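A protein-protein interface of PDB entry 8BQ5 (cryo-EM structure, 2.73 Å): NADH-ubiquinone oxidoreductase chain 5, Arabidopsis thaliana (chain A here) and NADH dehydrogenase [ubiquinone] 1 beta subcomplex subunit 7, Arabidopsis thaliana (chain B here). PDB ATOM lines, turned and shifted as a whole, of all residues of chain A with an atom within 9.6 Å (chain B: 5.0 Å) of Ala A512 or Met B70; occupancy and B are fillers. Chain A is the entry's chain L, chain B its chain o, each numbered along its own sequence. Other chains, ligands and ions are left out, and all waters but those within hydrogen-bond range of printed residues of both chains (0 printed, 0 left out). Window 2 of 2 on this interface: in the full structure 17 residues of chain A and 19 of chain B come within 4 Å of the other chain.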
ATOM      1  N   GLU A 406     -34.317 -22.047  -0.215  1.00  0.00           N
ATOM      2  CA  GLU A 406     -33.362 -22.746   0.682  1.00  0.00           C
ATOM      3  C   GLU A 406     -32.630 -21.712   1.534  1.00  0.00           C
ATOM      4  O   GLU A 406     -32.380 -22.013   2.709  1.00  0.00           O
ATOM      5  CB  GLU A 406     -32.363 -23.572  -0.129  1.00  0.00           C
ATOM      6  CG  GLU A 406     -32.938 -24.850  -0.706  1.00  0.00           C
ATOM      7  CD  GLU A 406     -31.961 -25.626  -1.573  1.00  0.00           C
ATOM      8  OE1 GLU A 406     -32.384 -26.128  -2.635  1.00  0.00           O
ATOM      9  OE2 GLU A 406     -30.779 -25.735  -1.181  1.00  0.00           O
ATOM     10  N   TYR A 409     -34.968 -20.447   4.253  1.00  0.00           N
ATOM     11  CA  TYR A 409     -35.068 -21.396   5.357  1.00  0.00           C
ATOM     12  C   TYR A 409     -33.892 -21.248   6.312  1.00  0.00           C
ATOM     13  O   TYR A 409     -34.062 -21.298   7.535  1.00  0.00           O
ATOM     14  CB  TYR A 409     -35.145 -22.825   4.823  1.00  0.00           C
ATOM     15  CG  TYR A 409     -35.150 -23.869   5.914  1.00  0.00           C
ATOM     16  CD1 TYR A 409     -36.309 -24.152   6.618  1.00  0.00           C
ATOM     17  CD2 TYR A 409     -33.994 -24.567   6.243  1.00  0.00           C
ATOM     18  CE1 TYR A 409     -36.322 -25.099   7.619  1.00  0.00           C
ATOM     19  CE2 TYR A 409     -33.997 -25.516   7.243  1.00  0.00           C
ATOM     20  CZ  TYR A 409     -35.165 -25.779   7.928  1.00  0.00           C
ATOM     21  OH  TYR A 409     -35.182 -26.724   8.926  1.00  0.00           O
ATOM     22  N   THR A 410     -32.690 -21.054   5.767  1.00  0.00           N
ATOM     23  CA  THR A 410     -31.467 -20.935   6.547  1.00  0.00           C
ATOM     24  C   THR A 410     -31.365 -19.612   7.300  1.00  0.00           C
ATOM     25  O   THR A 410     -30.461 -19.454   8.125  1.00  0.00           O
ATOM     26  CB  THR A 410     -30.260 -21.116   5.622  1.00  0.00           C
ATOM     27  OG1 THR A 410     -30.565 -22.118   4.645  1.00  0.00           O
ATOM     28  CG2 THR A 410     -29.028 -21.554   6.401  1.00  0.00           C
ATOM     29  N   TYR A 412     -32.521 -17.625  10.211  1.00  0.00           N
ATOM     30  CA  TYR A 412     -33.246 -17.903  11.486  1.00  0.00           C
ATOM     31  C   TYR A 412     -33.633 -16.580  12.150  1.00  0.00           C
ATOM     32  O   TYR A 412     -33.008 -16.197  13.149  1.00  0.00           O
ATOM     33  CB  TYR A 412     -32.452 -18.873  12.374  1.00  0.00           C
ATOM     34  CG  TYR A 412     -32.424 -20.275  11.823  1.00  0.00           C
ATOM     35  CD1 TYR A 412     -31.492 -20.651  10.872  1.00  0.00           C
ATOM     36  CD2 TYR A 412     -33.354 -21.219  12.221  1.00  0.00           C
ATOM     37  CE1 TYR A 412     -31.475 -21.930  10.341  1.00  0.00           C
ATOM     38  CE2 TYR A 412     -33.352 -22.503  11.703  1.00  0.00           C
ATOM     39  CZ  TYR A 412     -32.411 -22.858  10.755  1.00  0.00           C
ATOM     40  OH  TYR A 412     -32.400 -24.118  10.237  1.00  0.00           O
ATOM     41  N   ILE A 505     -24.797 -16.802   4.454  1.00  0.00           N
ATOM     42  CA  ILE A 505     -25.529 -18.009   4.815  1.00  0.00           C
ATOM     43  C   ILE A 505     -25.587 -19.023   3.683  1.00  0.00           C
ATOM     44  O   ILE A 505     -26.370 -19.970   3.758  1.00  0.00           O
ATOM     45  CB  ILE A 505     -26.955 -17.676   5.298  1.00  0.00           C
ATOM     46  CG1 ILE A 505     -27.745 -16.981   4.187  1.00  0.00           C
ATOM     47  CG2 ILE A 505     -26.906 -16.812   6.546  1.00  0.00           C
ATOM     48  CD1 ILE A 505     -29.219 -16.808   4.491  1.00  0.00           C
ATOM     49  N   LEU A 506     -24.788 -18.854   2.628  1.00  0.00           N
ATOM     50  CA  LEU A 506     -24.891 -19.739   1.472  1.00  0.00           C
ATOM     51  C   LEU A 506     -24.393 -21.141   1.801  1.00  0.00           C
ATOM     52  O   LEU A 506     -25.023 -22.138   1.429  1.00  0.00           O
ATOM     53  CB  LEU A 506     -24.117 -19.149   0.295  1.00  0.00           C
ATOM     54  CG  LEU A 506     -24.277 -19.856  -1.051  1.00  0.00           C
ATOM     55  CD1 LEU A 506     -25.725 -19.825  -1.503  1.00  0.00           C
ATOM     56  CD2 LEU A 506     -23.383 -19.201  -2.086  1.00  0.00           C
ATOM     57  N   ALA A 507     -23.258 -21.236   2.496  1.00  0.00           N
ATOM     58  CA  ALA A 507     -22.703 -22.543   2.834  1.00  0.00           C
ATOM     59  C   ALA A 507     -23.682 -23.355   3.670  1.00  0.00           C
ATOM     60  O   ALA A 507     -23.979 -24.513   3.354  1.00  0.00           O
ATOM     61  CB  ALA A 507     -21.376 -22.372   3.575  1.00  0.00           C
ATOM     62  N   GLU A 508     -24.215 -22.752   4.735  1.00  0.00           N
ATOM     63  CA  GLU A 508     -25.150 -23.460   5.601  1.00  0.00           C
ATOM     64  C   GLU A 508     -26.425 -23.849   4.865  1.00  0.00           C
ATOM     65  O   GLU A 508     -27.061 -24.849   5.218  1.00  0.00           O
ATOM     66  CB  GLU A 508     -25.476 -22.602   6.821  1.00  0.00           C
ATOM     67  CG  GLU A 508     -24.252 -22.210   7.626  1.00  0.00           C
ATOM     68  CD  GLU A 508     -23.751 -20.819   7.297  1.00  0.00           C
ATOM     69  OE1 GLU A 508     -23.626 -20.500   6.097  1.00  0.00           O
ATOM     70  OE2 GLU A 508     -23.470 -20.051   8.239  1.00  0.00           O
ATOM     71  N   SER A 509     -26.821 -23.079   3.851  1.00  0.00           N
ATOM     72  CA  SER A 509     -28.043 -23.407   3.126  1.00  0.00           C
ATOM     73  C   SER A 509     -27.891 -24.703   2.336  1.00  0.00           C
ATOM     74  O   SER A 509     -28.831 -25.501   2.260  1.00  0.00           O
ATOM     75  CB  SER A 509     -28.439 -22.250   2.207  1.00  0.00           C
ATOM     76  OG  SER A 509     -27.876 -22.396   0.917  1.00  0.00           O
ATOM     77  N   GLU A 510     -26.717 -24.933   1.748  1.00  0.00           N
ATOM     78  CA  GLU A 510     -26.510 -26.110   0.914  1.00  0.00           C
ATOM     79  C   GLU A 510     -25.922 -27.297   1.670  1.00  0.00           C
ATOM     80  O   GLU A 510     -25.755 -28.363   1.071  1.00  0.00           O
ATOM     81  CB  GLU A 510     -25.607 -25.761  -0.276  1.00  0.00           C
ATOM     82  CG  GLU A 510     -24.145 -25.512   0.079  1.00  0.00           C
ATOM     83  CD  GLU A 510     -23.223 -25.592  -1.129  1.00  0.00           C
ATOM     84  OE1 GLU A 510     -23.411 -26.493  -1.972  1.00  0.00           O
ATOM     85  OE2 GLU A 510     -22.309 -24.748  -1.235  1.00  0.00           O
ATOM     86  N   PHE A 511     -25.612 -27.151   2.960  1.00  0.00           N
ATOM     87  CA  PHE A 511     -24.970 -28.235   3.696  1.00  0.00           C
ATOM     88  C   PHE A 511     -25.718 -28.588   4.977  1.00  0.00           C
ATOM     89  O   PHE A 511     -25.739 -29.754   5.385  1.00  0.00           O
ATOM     90  CB  PHE A 511     -23.523 -27.868   4.032  1.00  0.00           C
ATOM     91  CG  PHE A 511     -22.642 -27.697   2.829  1.00  0.00           C
ATOM     92  CD1 PHE A 511     -22.689 -28.599   1.781  1.00  0.00           C
ATOM     93  CD2 PHE A 511     -21.755 -26.637   2.754  1.00  0.00           C
ATOM     94  CE1 PHE A 511     -21.875 -28.442   0.678  1.00  0.00           C
ATOM     95  CE2 PHE A 511     -20.938 -26.475   1.654  1.00  0.00           C
ATOM     96  CZ  PHE A 511     -20.999 -27.381   0.614  1.00  0.00           C
ATOM     97  N   ALA A 512     -26.321 -27.594   5.624  1.00  0.00           N
ATOM     98  CA  ALA A 512     -26.988 -27.787   6.905  1.00  0.00           C
ATOM     99  C   ALA A 512     -28.503 -27.875   6.780  1.00  0.00           C
ATOM    100  O   ALA A 512     -29.200 -27.823   7.798  1.00  0.00           O
ATOM    101  CB  ALA A 512     -26.613 -26.663   7.871  1.00  0.00           C
ATOM    102  N   ALA A 513     -29.028 -28.009   5.564  1.00  0.00           N
ATOM    103  CA  ALA A 513     -30.480 -28.048   5.456  1.00  0.00           C
ATOM    104  C   ALA A 513     -30.971 -29.483   5.297  1.00  0.00           C
ATOM    105  O   ALA A 513     -30.302 -30.302   4.657  1.00  0.00           O
ATOM    106  CB  ALA A 513     -30.954 -27.221   4.269  1.00  0.00           C
ATOM    107  N   PRO A 514     -32.128 -29.803   5.875  1.00  0.00           N
ATOM    108  CA  PRO A 514     -32.714 -31.129   5.656  1.00  0.00           C
ATOM    109  C   PRO A 514     -33.019 -31.352   4.183  1.00  0.00           C
ATOM    110  O   PRO A 514     -33.383 -30.425   3.456  1.00  0.00           O
ATOM    111  CB  PRO A 514     -33.995 -31.097   6.498  1.00  0.00           C
ATOM    112  CG  PRO A 514     -33.764 -30.018   7.504  1.00  0.00           C
ATOM    113  CD  PRO A 514     -32.918 -28.995   6.816  1.00  0.00           C
ATOM    114  N   THR A 515     -32.859 -32.602   3.744  1.00  0.00           N
ATOM    115  CA  THR A 515     -33.140 -32.935   2.353  1.00  0.00           C
ATOM    116  C   THR A 515     -34.615 -32.765   2.021  1.00  0.00           C
ATOM    117  O   THR A 515     -34.978 -32.663   0.845  1.00  0.00           O
ATOM    118  CB  THR A 515     -32.701 -34.368   2.053  1.00  0.00           C
ATOM    119  OG1 THR A 515     -33.163 -35.235   3.094  1.00  0.00           O
ATOM    120  CG2 THR A 515     -31.183 -34.455   1.960  1.00  0.00           C
ATOM    121  N   ILE A 516     -35.481 -32.743   3.036  1.00  0.00           N
ATOM    122  CA  ILE A 516     -36.903 -32.527   2.789  1.00  0.00           C
ATOM    123  C   ILE A 516     -37.145 -31.098   2.315  1.00  0.00           C
ATOM    124  O   ILE A 516     -38.045 -30.837   1.507  1.00  0.00           O
ATOM    125  CB  ILE A 516     -37.732 -32.865   4.042  1.00  0.00           C
ATOM    126  CG1 ILE A 516     -39.211 -32.978   3.673  1.00  0.00           C
ATOM    127  CG2 ILE A 516     -37.531 -31.825   5.138  1.00  0.00           C
ATOM    128  CD1 ILE A 516     -39.467 -33.859   2.467  1.00  0.00           C
ATOM    129  N   ILE A 517     -36.346 -30.150   2.813  1.00  0.00           N
ATOM    130  CA  ILE A 517     -36.481 -28.760   2.389  1.00  0.00           C
ATOM    131  C   ILE A 517     -36.154 -28.617   0.912  1.00  0.00           C
ATOM    132  O   ILE A 517     -36.873 -27.939   0.169  1.00  0.00           O
ATOM    133  CB  ILE A 517     -35.589 -27.842   3.251  1.00  0.00           C
ATOM    134  CG1 ILE A 517     -36.042 -27.869   4.710  1.00  0.00           C
ATOM    135  CG2 ILE A 517     -35.623 -26.412   2.722  1.00  0.00           C
ATOM    136  CD1 ILE A 517     -37.527 -27.687   4.884  1.00  0.00           C
ATOM    137  N   LYS A 518     -35.079 -29.260   0.456  1.00  0.00           N
ATOM    138  CA  LYS A 518     -34.658 -29.130  -0.933  1.00  0.00           C
ATOM    139  C   LYS A 518     -35.654 -29.732  -1.915  1.00  0.00           C
ATOM    140  O   LYS A 518     -35.537 -29.488  -3.122  1.00  0.00           O
ATOM    141  CB  LYS A 518     -33.287 -29.780  -1.136  1.00  0.00           C
ATOM    142  CG  LYS A 518     -32.208 -29.289  -0.183  1.00  0.00           C
ATOM    143  CD  LYS A 518     -30.996 -30.212  -0.204  1.00  0.00           C
ATOM    144  CE  LYS A 518     -29.735 -29.478  -0.645  1.00  0.00           C
ATOM    145  NZ  LYS A 518     -29.287 -28.468   0.354  1.00  0.00           N
ATOM    146  N   VAL B  66     -19.215 -26.340   8.466  1.00  0.00           N
ATOM    147  CA  VAL B  66     -20.610 -26.269   8.889  1.00  0.00           C
ATOM    148  C   VAL B  66     -20.940 -27.399   9.858  1.00  0.00           C
ATOM    149  O   VAL B  66     -21.620 -27.190  10.872  1.00  0.00           O
ATOM    150  CB  VAL B  66     -21.530 -26.279   7.654  1.00  0.00           C
ATOM    151  CG1 VAL B  66     -22.873 -26.911   7.978  1.00  0.00           C
ATOM    152  CG2 VAL B  66     -21.717 -24.867   7.128  1.00  0.00           C
ATOM    153  N   MET B  67     -20.464 -28.613   9.566  1.00  0.00           N
ATOM    154  CA  MET B  67     -20.736 -29.748  10.444  1.00  0.00           C
ATOM    155  C   MET B  67     -20.132 -29.533  11.825  1.00  0.00           C
ATOM    156  O   MET B  67     -20.778 -29.810  12.842  1.00  0.00           O
ATOM    157  CB  MET B  67     -20.200 -31.036   9.823  1.00  0.00           C
ATOM    158  CG  MET B  67     -20.912 -31.466   8.554  1.00  0.00           C
ATOM    159  SD  MET B  67     -22.672 -31.760   8.789  1.00  0.00           S
ATOM    160  CE  MET B  67     -23.354 -30.499   7.719  1.00  0.00           C
ATOM    161  N   GLU B  68     -18.894 -29.029  11.878  1.00  0.00           N
ATOM    162  CA  GLU B  68     -18.279 -28.703  13.162  1.00  0.00           C
ATOM    163  C   GLU B  68     -19.136 -27.719  13.950  1.00  0.00           C
ATOM    164  O   GLU B  68     -19.378 -27.917  15.147  1.00  0.00           O
ATOM    165  CB  GLU B  68     -16.861 -28.147  12.963  1.00  0.00           C
ATOM    166  CG  GLU B  68     -16.127 -27.851  14.247  1.00  0.00           C
ATOM    167  CD  GLU B  68     -14.734 -27.357  14.033  1.00  0.00           C
ATOM    168  OE1 GLU B  68     -14.313 -27.196  12.866  1.00  0.00           O
ATOM    169  OE2 GLU B  68     -14.043 -27.127  15.035  1.00  0.00           O
ATOM    170  N   ARG B  69     -19.620 -26.660  13.294  1.00  0.00           N
ATOM    171  CA  ARG B  69     -20.460 -25.690  13.979  1.00  0.00           C
ATOM    172  C   ARG B  69     -21.831 -26.269  14.273  1.00  0.00           C
ATOM    173  O   ARG B  69     -22.523 -25.790  15.177  1.00  0.00           O
ATOM    174  CB  ARG B  69     -20.575 -24.414  13.146  1.00  0.00           C
ATOM    175  CG  ARG B  69     -19.408 -23.461  13.303  1.00  0.00           C
ATOM    176  CD  ARG B  69     -19.489 -22.348  12.287  1.00  0.00           C
ATOM    177  NE  ARG B  69     -20.834 -21.793  12.228  1.00  0.00           N
ATOM    178  CZ  ARG B  69     -21.502 -21.577  11.104  1.00  0.00           C
ATOM    179  NH1 ARG B  69     -20.975 -21.855   9.923  1.00  0.00           N
ATOM    180  NH2 ARG B  69     -22.731 -21.077  11.166  1.00  0.00           N
ATOM    181  N   MET B  70     -22.245 -27.289  13.520  1.00  0.00           N
ATOM    182  CA  MET B  70     -23.456 -28.014  13.880  1.00  0.00           C
ATOM    183  C   MET B  70     -23.219 -28.896  15.098  1.00  0.00           C
ATOM    184  O   MET B  70     -24.067 -28.967  15.995  1.00  0.00           O
ATOM    185  CB  MET B  70     -23.941 -28.850  12.698  1.00  0.00           C
ATOM    186  CG  MET B  70     -24.805 -28.093  11.712  1.00  0.00           C
ATOM    187  SD  MET B  70     -25.197 -29.098  10.274  1.00  0.00           S
ATOM    188  CE  MET B  70     -26.926 -29.452  10.564  1.00  0.00           C
ATOM    189  N   LEU B  71     -22.069 -29.576  15.147  1.00  0.00           N
ATOM    190  CA  LEU B  71     -21.730 -30.369  16.323  1.00  0.00           C
ATOM    191  C   LEU B  71     -21.570 -29.487  17.553  1.00  0.00           C
ATOM    192  O   LEU B  71     -21.982 -29.867  18.654  1.00  0.00           O
ATOM    193  CB  LEU B  71     -20.454 -31.174  16.071  1.00  0.00           C
ATOM    194  CG  LEU B  71     -20.482 -32.265  14.993  1.00  0.00           C
ATOM    195  CD1 LEU B  71     -19.102 -32.869  14.766  1.00  0.00           C
ATOM    196  CD2 LEU B  71     -21.511 -33.347  15.302  1.00  0.00           C
ATOM    197  N   ALA B  72     -20.975 -28.304  17.383  1.00  0.00           N
ATOM    198  CA  ALA B  72     -20.799 -27.394  18.509  1.00  0.00           C
ATOM    199  C   ALA B  72     -22.143 -26.989  19.099  1.00  0.00           C
ATOM    200  O   ALA B  72     -22.315 -26.959  20.323  1.00  0.00           O
ATOM    201  CB  ALA B  72     -20.006 -26.164  18.069  1.00  0.00           C
ATOM    202  N   MET B  73     -23.118 -26.683  18.239  1.00  0.00           N
ATOM    203  CA  MET B  73     -24.433 -26.287  18.732  1.00  0.00           C
ATOM    204  C   MET B  73     -25.171 -27.455  19.375  1.00  0.00           C
ATOM    205  O   MET B  73     -25.945 -27.249  20.317  1.00  0.00           O
ATOM    206  CB  MET B  73     -25.260 -25.682  17.594  1.00  0.00           C
ATOM    207  CG  MET B  73     -26.700 -25.312  17.958  1.00  0.00           C
ATOM    208  SD  MET B  73     -27.017 -24.062  19.236  1.00  0.00           S
ATOM    209  CE  MET B  73     -25.481 -23.146  19.360  1.00  0.00           C
ATOM    210  N   LYS B  74     -24.937 -28.677  18.895  1.00  0.00           N
ATOM    211  CA  LYS B  74     -25.547 -29.849  19.516  1.00  0.00           C
ATOM    212  C   LYS B  74     -25.148 -29.952  20.982  1.00  0.00           C
ATOM    213  O   LYS B  74     -25.985 -30.231  21.847  1.00  0.00           O
ATOM    214  CB  LYS B  74     -25.143 -31.110  18.746  1.00  0.00           C
ATOM    215  CG  LYS B  74     -25.694 -31.219  17.327  1.00  0.00           C
ATOM    216  CD  LYS B  74     -25.231 -32.485  16.618  1.00  0.00           C
ATOM    217  CE  LYS B  74     -25.807 -32.592  15.217  1.00  0.00           C
ATOM    218  NZ  LYS B  74     -25.335 -33.818  14.514  1.00  0.00           N
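NH2 of Arg B69 lies within salt-bridge range of OE2 of Glu A508, at 3.2 Å.
Among the printed residues, merely in contact across the chains: Glu A508 with Val B66 (3.7 Å), Phe A511 with Met B67 (3.4 Å), Ala A512 with Val B66 (3.7 Å) and Ala A512 with Met B70 (3.7 Å).
Glu A406 touches none of the printed residues of chain B.
Of the printed residues of chain B, Glu A508 touches Val B66 (3.7 Å) and Arg B69 (3.2 Å).
Of the printed residues of chain B, Phe A511 touches Met B67 (3.4 Å).
Of the printed residues of chain B, Ala A512 touches Val B66 (3.7 Å) and Met B70 (3.7 Å).
Lys A518 touches none of the printed residues of chain B.
Printed residues of chain A within 4 Å of Val B66: Glu A508 (3.7 Å) and Ala A512 (3.7 Å).
Of the printed residues of chain A, Arg B69 touches Glu A508 (3.2 Å).
Printed residues of chain A within 4 Å of Met B70: Ala A512.
The nearest residue of chain A that does not touch Met B70 is Phe A511 (5.0 Å).
Of the 9 printed residues of chain B, 4 touch a printed residue of chain A.
Hydrophobic or aromatic side chains of chain B within 4 Å of the printed part of chain A: Val B66, Met B67 and Met B70.
Of the 18 printed residues of chain A, 3 touch a printed residue of chain B.
Printed residues of chain A that touch a printed residue of chain B: Glu A508, Phe A511 and Ala A512.
Among the printed residues, Asp or Glu carboxylates within 4 Å of a Lys or Arg side-chain nitrogen of the other chain: Glu A508 with Arg B69 (3.2 Å).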
